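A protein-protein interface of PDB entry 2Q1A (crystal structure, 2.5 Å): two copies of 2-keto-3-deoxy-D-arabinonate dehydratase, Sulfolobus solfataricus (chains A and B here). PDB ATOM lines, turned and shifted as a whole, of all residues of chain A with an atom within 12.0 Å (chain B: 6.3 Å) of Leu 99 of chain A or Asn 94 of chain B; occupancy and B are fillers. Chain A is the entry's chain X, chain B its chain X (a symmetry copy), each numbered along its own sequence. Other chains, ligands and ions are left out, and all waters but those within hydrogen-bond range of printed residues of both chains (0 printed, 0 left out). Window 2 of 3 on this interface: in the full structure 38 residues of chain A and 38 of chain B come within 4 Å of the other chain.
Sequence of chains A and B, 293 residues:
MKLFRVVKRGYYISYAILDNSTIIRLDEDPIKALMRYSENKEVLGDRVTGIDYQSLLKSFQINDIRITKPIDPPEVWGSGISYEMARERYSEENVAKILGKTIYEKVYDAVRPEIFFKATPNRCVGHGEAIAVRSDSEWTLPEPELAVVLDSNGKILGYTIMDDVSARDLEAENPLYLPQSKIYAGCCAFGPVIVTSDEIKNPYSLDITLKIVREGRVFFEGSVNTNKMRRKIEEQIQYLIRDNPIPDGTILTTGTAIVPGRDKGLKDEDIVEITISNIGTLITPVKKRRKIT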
ATOM      1  N   VAL A  95     -12.798   0.360 -12.516  1.00  0.00           N
ATOM      2  CA  VAL A  95     -13.934  -0.559 -12.607  1.00  0.00           C
ATOM      3  C   VAL A  95     -13.812  -1.705 -11.615  1.00  0.00           C
ATOM      4  O   VAL A  95     -12.705  -2.161 -11.315  1.00  0.00           O
ATOM      5  CB  VAL A  95     -14.096  -1.171 -14.019  1.00  0.00           C
ATOM      6  CG1 VAL A  95     -15.065  -0.357 -14.844  1.00  0.00           C
ATOM      7  CG2 VAL A  95     -12.744  -1.330 -14.714  1.00  0.00           C
ATOM      8  N   ALA A  96     -14.956  -2.161 -11.112  1.00  0.00           N
ATOM      9  CA  ALA A  96     -15.014  -3.327 -10.243  1.00  0.00           C
ATOM     10  C   ALA A  96     -14.719  -4.576 -11.056  1.00  0.00           C
ATOM     11  O   ALA A  96     -15.246  -4.742 -12.160  1.00  0.00           O
ATOM     12  CB  ALA A  96     -16.378  -3.431  -9.589  1.00  0.00           C
ATOM     13  N   LYS A  97     -13.871  -5.445 -10.515  1.00  0.00           N
ATOM     14  CA  LYS A  97     -13.497  -6.672 -11.217  1.00  0.00           C
ATOM     15  C   LYS A  97     -13.457  -7.930 -10.340  1.00  0.00           C
ATOM     16  O   LYS A  97     -13.085  -7.874  -9.167  1.00  0.00           O
ATOM     17  CB  LYS A  97     -12.195  -6.483 -12.019  1.00  0.00           C
ATOM     18  CG  LYS A  97     -11.143  -5.580 -11.373  1.00  0.00           C
ATOM     19  CD  LYS A  97     -10.556  -4.570 -12.374  1.00  0.00           C
ATOM     20  CE  LYS A  97      -9.715  -5.222 -13.476  1.00  0.00           C
ATOM     21  NZ  LYS A  97      -9.135  -4.209 -14.411  1.00  0.00           N
ATOM     22  N   ILE A  98     -13.882  -9.047 -10.933  1.00  0.00           N
ATOM     23  CA  ILE A  98     -13.845 -10.372 -10.309  1.00  0.00           C
ATOM     24  C   ILE A  98     -12.638 -11.127 -10.862  1.00  0.00           C
ATOM     25  O   ILE A  98     -12.658 -11.579 -12.012  1.00  0.00           O
ATOM     26  CB  ILE A  98     -15.132 -11.210 -10.623  1.00  0.00           C
ATOM     27  CG1 ILE A  98     -16.422 -10.381 -10.463  1.00  0.00           C
ATOM     28  CG2 ILE A  98     -15.155 -12.521  -9.814  1.00  0.00           C
ATOM     29  CD1 ILE A  98     -16.837 -10.080  -9.034  1.00  0.00           C
ATOM     30  N   LEU A  99     -11.598 -11.260 -10.036  1.00  0.00           N
ATOM     31  CA  LEU A  99     -10.322 -11.886 -10.425  1.00  0.00           C
ATOM     32  C   LEU A  99      -9.791 -11.399 -11.783  1.00  0.00           C
ATOM     33  O   LEU A  99      -9.585 -12.196 -12.703  1.00  0.00           O
ATOM     34  CB  LEU A  99     -10.411 -13.428 -10.403  1.00  0.00           C
ATOM     35  CG  LEU A  99     -10.661 -14.281  -9.146  1.00  0.00           C
ATOM     36  CD1 LEU A  99     -10.272 -13.586  -7.827  1.00  0.00           C
ATOM     37  CD2 LEU A  99     -12.104 -14.763  -9.095  1.00  0.00           C
ATOM     38  N   GLY A 100      -9.588 -10.087 -11.903  1.00  0.00           N
ATOM     39  CA  GLY A 100      -9.003  -9.494 -13.111  1.00  0.00           C
ATOM     40  C   GLY A 100      -9.979  -9.141 -14.222  1.00  0.00           C
ATOM     41  O   GLY A 100      -9.692  -8.276 -15.057  1.00  0.00           O
ATOM     42  N   LYS A 101     -11.129  -9.811 -14.234  1.00  0.00           N
ATOM     43  CA  LYS A 101     -12.171  -9.595 -15.236  1.00  0.00           C
ATOM     44  C   LYS A 101     -13.244  -8.671 -14.654  1.00  0.00           C
ATOM     45  O   LYS A 101     -13.681  -8.873 -13.519  1.00  0.00           O
ATOM     46  CB  LYS A 101     -12.784 -10.942 -15.622  1.00  0.00           C
ATOM     47  CG  LYS A 101     -13.145 -11.086 -17.083  1.00  0.00           C
ATOM     48  CD  LYS A 101     -13.377 -12.549 -17.440  1.00  0.00           C
ATOM     49  CE  LYS A 101     -13.324 -12.773 -18.948  1.00  0.00           C
ATOM     50  NZ  LYS A 101     -13.403 -14.222 -19.295  1.00  0.00           N
ATOM     51  N   THR A 102     -13.661  -7.661 -15.420  1.00  0.00           N
ATOM     52  CA  THR A 102     -14.640  -6.680 -14.932  1.00  0.00           C
ATOM     53  C   THR A 102     -16.051  -7.264 -14.819  1.00  0.00           C
ATOM     54  O   THR A 102     -16.410  -8.195 -15.548  1.00  0.00           O
ATOM     55  CB  THR A 102     -14.703  -5.406 -15.807  1.00  0.00           C
ATOM     56  OG1 THR A 102     -15.333  -5.708 -17.056  1.00  0.00           O
ATOM     57  CG2 THR A 102     -13.317  -4.836 -16.051  1.00  0.00           C
ATOM     58  N   ILE A 103     -16.842  -6.694 -13.910  1.00  0.00           N
ATOM     59  CA  ILE A 103     -18.224  -7.126 -13.661  1.00  0.00           C
ATOM     60  C   ILE A 103     -19.094  -7.166 -14.928  1.00  0.00           C
ATOM     61  O   ILE A 103     -19.894  -8.087 -15.103  1.00  0.00           O
ATOM     62  CB  ILE A 103     -18.911  -6.279 -12.548  1.00  0.00           C
ATOM     63  CG1 ILE A 103     -18.797  -4.778 -12.848  1.00  0.00           C
ATOM     64  CG2 ILE A 103     -18.315  -6.603 -11.180  1.00  0.00           C
ATOM     65  CD1 ILE A 103     -19.711  -3.896 -12.012  1.00  0.00           C
ATOM     66  N   TYR A 104     -18.915  -6.175 -15.804  1.00  0.00           N
ATOM     67  CA  TYR A 104     -19.652  -6.085 -17.070  1.00  0.00           C
ATOM     68  C   TYR A 104     -19.167  -7.139 -18.060  1.00  0.00           C
ATOM     69  O   TYR A 104     -19.959  -7.732 -18.798  1.00  0.00           O
ATOM     70  CB  TYR A 104     -19.528  -4.676 -17.675  1.00  0.00           C
ATOM     71  CG  TYR A 104     -19.900  -3.569 -16.710  1.00  0.00           C
ATOM     72  CD1 TYR A 104     -21.235  -3.239 -16.478  1.00  0.00           C
ATOM     73  CD2 TYR A 104     -18.918  -2.861 -16.016  1.00  0.00           C
ATOM     74  CE1 TYR A 104     -21.583  -2.235 -15.586  1.00  0.00           C
ATOM     75  CE2 TYR A 104     -19.259  -1.851 -15.121  1.00  0.00           C
ATOM     76  CZ  TYR A 104     -20.593  -1.549 -14.912  1.00  0.00           C
ATOM     77  OH  TYR A 104     -20.946  -0.558 -14.029  1.00  0.00           O
ATOM     78  N   GLU A 105     -17.855  -7.361 -18.057  1.00  0.00           N
ATOM     79  CA  GLU A 105     -17.213  -8.364 -18.898  1.00  0.00           C
ATOM     80  C   GLU A 105     -17.728  -9.758 -18.523  1.00  0.00           C
ATOM     81  O   GLU A 105     -18.108 -10.548 -19.395  1.00  0.00           O
ATOM     82  CB  GLU A 105     -15.700  -8.277 -18.702  1.00  0.00           C
ATOM     83  CG  GLU A 105     -14.853  -8.578 -19.916  1.00  0.00           C
ATOM     84  CD  GLU A 105     -13.427  -8.073 -19.744  1.00  0.00           C
ATOM     85  OE1 GLU A 105     -13.171  -6.887 -20.050  1.00  0.00           O
ATOM     86  OE2 GLU A 105     -12.560  -8.859 -19.302  1.00  0.00           O
ATOM     87  N   LYS A 106     -17.759 -10.030 -17.219  1.00  0.00           N
ATOM     88  CA  LYS A 106     -18.238 -11.301 -16.676  1.00  0.00           C
ATOM     89  C   LYS A 106     -19.717 -11.589 -17.003  1.00  0.00           C
ATOM     90  O   LYS A 106     -20.051 -12.694 -17.440  1.00  0.00           O
ATOM     91  CB  LYS A 106     -17.995 -11.343 -15.161  1.00  0.00           C
ATOM     92  CG  LYS A 106     -18.097 -12.729 -14.518  1.00  0.00           C
ATOM     93  CD  LYS A 106     -16.877 -13.605 -14.813  1.00  0.00           C
ATOM     94  CE  LYS A 106     -16.922 -14.911 -14.023  1.00  0.00           C
ATOM     95  NZ  LYS A 106     -15.754 -15.774 -14.343  1.00  0.00           N
ATOM     96  N   VAL A 107     -20.584 -10.591 -16.808  1.00  0.00           N
ATOM     97  CA  VAL A 107     -22.028 -10.755 -17.019  1.00  0.00           C
ATOM     98  C   VAL A 107     -22.433 -10.894 -18.495  1.00  0.00           C
ATOM     99  O   VAL A 107     -23.478 -11.475 -18.801  1.00  0.00           O
ATOM    100  CB  VAL A 107     -22.855  -9.639 -16.306  1.00  0.00           C
ATOM    101  CG1 VAL A 107     -22.986  -8.388 -17.176  1.00  0.00           C
ATOM    102  CG2 VAL A 107     -24.229 -10.157 -15.916  1.00  0.00           C
ATOM    103  N   PRO A 175     -20.394   0.190  -8.265  1.00  0.00           N
ATOM    104  CA  PRO A 175     -21.585  -0.494  -8.806  1.00  0.00           C
ATOM    105  C   PRO A 175     -22.738  -0.646  -7.801  1.00  0.00           C
ATOM    106  O   PRO A 175     -23.858  -0.964  -8.201  1.00  0.00           O
ATOM    107  CB  PRO A 175     -21.050  -1.866  -9.233  1.00  0.00           C
ATOM    108  CG  PRO A 175     -19.764  -2.046  -8.466  1.00  0.00           C
ATOM    109  CD  PRO A 175     -19.191  -0.664  -8.318  1.00  0.00           C
ATOM    110  N   TYR B  90     -19.307 -11.018   3.050  1.00  0.00           N
ATOM    111  CA  TYR B  90     -18.545 -11.793   2.062  1.00  0.00           C
ATOM    112  C   TYR B  90     -17.093 -11.298   1.956  1.00  0.00           C
ATOM    113  O   TYR B  90     -16.780 -10.403   1.165  1.00  0.00           O
ATOM    114  CB  TYR B  90     -19.258 -11.850   0.695  1.00  0.00           C
ATOM    115  CG  TYR B  90     -18.943 -13.097  -0.103  1.00  0.00           C
ATOM    116  CD1 TYR B  90     -19.302 -14.364   0.370  1.00  0.00           C
ATOM    117  CD2 TYR B  90     -18.290 -13.013  -1.335  1.00  0.00           C
ATOM    118  CE1 TYR B  90     -19.010 -15.519  -0.360  1.00  0.00           C
ATOM    119  CE2 TYR B  90     -17.991 -14.163  -2.076  1.00  0.00           C
ATOM    120  CZ  TYR B  90     -18.356 -15.411  -1.581  1.00  0.00           C
ATOM    121  OH  TYR B  90     -18.069 -16.545  -2.307  1.00  0.00           O
ATOM    122  N   GLU B  92     -14.439 -13.549   1.559  1.00  0.00           N
ATOM    123  CA  GLU B  92     -13.729 -14.494   0.699  1.00  0.00           C
ATOM    124  C   GLU B  92     -13.415 -13.905  -0.677  1.00  0.00           C
ATOM    125  O   GLU B  92     -14.235 -13.181  -1.244  1.00  0.00           O
ATOM    126  CB  GLU B  92     -14.550 -15.780   0.545  1.00  0.00           C
ATOM    127  CG  GLU B  92     -13.800 -16.928  -0.123  1.00  0.00           C
ATOM    128  CD  GLU B  92     -14.727 -17.902  -0.821  1.00  0.00           C
ATOM    129  OE1 GLU B  92     -15.358 -18.729  -0.126  1.00  0.00           O
ATOM    130  OE2 GLU B  92     -14.819 -17.842  -2.067  1.00  0.00           O
ATOM    131  N   GLU B  93     -12.225 -14.222  -1.194  1.00  0.00           N
ATOM    132  CA  GLU B  93     -11.820 -13.856  -2.559  1.00  0.00           C
ATOM    133  C   GLU B  93     -12.882 -14.246  -3.584  1.00  0.00           C
ATOM    134  O   GLU B  93     -13.671 -15.169  -3.352  1.00  0.00           O
ATOM    135  CB  GLU B  93     -10.471 -14.496  -2.926  1.00  0.00           C
ATOM    136  CG  GLU B  93      -9.265 -13.548  -2.864  1.00  0.00           C
ATOM    137  CD  GLU B  93      -8.680 -13.387  -1.461  1.00  0.00           C
ATOM    138  OE1 GLU B  93      -9.342 -12.773  -0.592  1.00  0.00           O
ATOM    139  OE2 GLU B  93      -7.542 -13.856  -1.234  1.00  0.00           O
ATOM    140  N   ASN B  94     -12.871 -13.548  -4.717  1.00  0.00           N
ATOM    141  CA  ASN B  94     -13.934 -13.601  -5.731  1.00  0.00           C
ATOM    142  C   ASN B  94     -14.857 -12.391  -5.645  1.00  0.00           C
ATOM    143  O   ASN B  94     -15.627 -12.135  -6.569  1.00  0.00           O
ATOM    144  CB  ASN B  94     -14.750 -14.904  -5.684  1.00  0.00           C
ATOM    145  CG  ASN B  94     -14.053 -16.059  -6.389  1.00  0.00           C
ATOM    146  OD1 ASN B  94     -14.566 -16.595  -7.372  1.00  0.00           O
ATOM    147  ND2 ASN B  94     -12.875 -16.442  -5.893  1.00  0.00           N
ATOM    148  N   VAL B  95     -14.774 -11.657  -4.536  1.00  0.00           N
ATOM    149  CA  VAL B  95     -15.494 -10.391  -4.382  1.00  0.00           C
ATOM    150  C   VAL B  95     -15.031  -9.354  -5.394  1.00  0.00           C
ATOM    151  O   VAL B  95     -13.857  -9.325  -5.770  1.00  0.00           O
ATOM    152  CB  VAL B  95     -15.333  -9.779  -2.971  1.00  0.00           C
ATOM    153  CG1 VAL B  95     -16.474 -10.199  -2.074  1.00  0.00           C
ATOM    154  CG2 VAL B  95     -13.973 -10.126  -2.366  1.00  0.00           C
ATOM    155  N   ALA B  96     -15.964  -8.510  -5.828  1.00  0.00           N
ATOM    156  CA  ALA B  96     -15.654  -7.392  -6.705  1.00  0.00           C
ATOM    157  C   ALA B  96     -14.877  -6.343  -5.927  1.00  0.00           C
ATOM    158  O   ALA B  96     -15.236  -6.011  -4.794  1.00  0.00           O
ATOM    159  CB  ALA B  96     -16.929  -6.795  -7.270  1.00  0.00           C
ATOM    160  N   LYS B  97     -13.810  -5.831  -6.533  1.00  0.00           N
ATOM    161  CA  LYS B  97     -12.974  -4.830  -5.871  1.00  0.00           C
ATOM    162  C   LYS B  97     -12.540  -3.661  -6.764  1.00  0.00           C
ATOM    163  O   LYS B  97     -12.290  -3.833  -7.958  1.00  0.00           O
ATOM    164  CB  LYS B  97     -11.779  -5.485  -5.153  1.00  0.00           C
ATOM    165  CG  LYS B  97     -11.167  -6.700  -5.855  1.00  0.00           C
ATOM    166  CD  LYS B  97     -10.920  -7.865  -4.882  1.00  0.00           C
ATOM    167  CE  LYS B  97      -9.831  -7.574  -3.844  1.00  0.00           C
ATOM    168  NZ  LYS B  97      -9.596  -8.739  -2.937  1.00  0.00           N
ATOM    169  N   ALA B 172     -23.088 -12.848  -4.549  1.00  0.00           N
ATOM    170  CA  ALA B 172     -21.663 -13.197  -4.512  1.00  0.00           C
ATOM    171  C   ALA B 172     -21.086 -13.497  -5.893  1.00  0.00           C
ATOM    172  O   ALA B 172     -19.958 -13.106  -6.184  1.00  0.00           O
ATOM    173  CB  ALA B 172     -21.430 -14.377  -3.573  1.00  0.00           C
ATOM    174  N   GLU B 173     -21.858 -14.185  -6.734  1.00  0.00           N
ATOM    175  CA  GLU B 173     -21.442 -14.513  -8.099  1.00  0.00           C
ATOM    176  C   GLU B 173     -21.119 -13.256  -8.913  1.00  0.00           C
ATOM    177  O   GLU B 173     -20.214 -13.269  -9.748  1.00  0.00           O
ATOM    178  CB  GLU B 173     -22.527 -15.335  -8.807  1.00  0.00           C
ATOM    179  CG  GLU B 173     -22.090 -15.959 -10.133  1.00  0.00           C
ATOM    180  CD  GLU B 173     -23.237 -16.582 -10.923  1.00  0.00           C
ATOM    181  OE1 GLU B 173     -24.275 -16.941 -10.318  1.00  0.00           O
ATOM    182  OE2 GLU B 173     -23.097 -16.722 -12.161  1.00  0.00           O
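The backbone carbonyl oxygen (O) of Lys 97 of chain B sits at hydrogen-bond distance from the backbone NH (N) of Lys 97 of chain A (3.4 Å).
Val 95 of chain A touches Lys 97 of chain B, and with the chains exchanged Lys 97 of chain A touches Val 95 of chain B.
Ala 96 of chain A touches Lys 97 of chain B, and with the chains exchanged Lys 97 of chain A touches Ala 96 of chain B.
Lys 97 of chain B touches its own counterpart, Lys 97 of chain A.
Of the 8 pairs that touch across the chains among the printed residues, 5 have their exchanged pair printed and touching as well.
Printed residues of chain B within 4 Å of Ala 96 of chain A: Lys 97 (3.6 Å).
Of the printed residues of chain B, Ile 98 of chain A touches Asn 94 and Ala 96.
Lys 106 of chain A touches none of the printed residues of chain B.
No residue of chain A comes within 4 Å of Glu 92 of chain B.
No residue of chain A comes within 4 Å of Glu 93 of chain B.
Printed residues of chain A within 4 Å of Asn 94 of chain B: Ile 98 (3.3 Å) and Leu 99 (3.5 Å).
Ala 96 of chain B touches two residues of chain A.
Printed residues of chain A within 4 Å of Lys 97 of chain B: Val 95, Ala 96 and Lys 97.
No residue of chain A comes within 4 Å of Ala 172 of chain B.
The nearest residue of chain B that does not touch Leu 99 of chain A is Glu 93 of chain B (5.0 Å).
Among the printed residues, merely in contact across the chains: Ile 98 of chain A with Asn 94 of chain B, Leu 99 of chain A with Asn 94 of chain B, Lys 97 of chain A with Ala 96 of chain B, Ala 96 of chain A with Lys 97 of chain B, Ile 98 of chain A with Ala 96 of chain B, Val 95 of chain A with Lys 97 of chain B and Lys 97 of chain A with Val 95 of chain B.
Of the 9 printed residues of chain B, 4 touch a printed residue of chain A.
Of the 14 printed residues of chain A, 5 touch a printed residue of chain B.
Hydrophobic or aromatic side chains of chain A within 4 Å of the printed part of chain B: Ile 98 and Leu 99.
Among the printed residues, 8 pairs touch across the chains.
Among the printed residues, no Asp or Glu carboxylate lies within 4 Å of a Lys or Arg side-chain nitrogen of the other chain.
O of Ala 96 of chain A lies within hydrogen-bond range of N of Ile 103 of chain A, 3.1 Å away.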
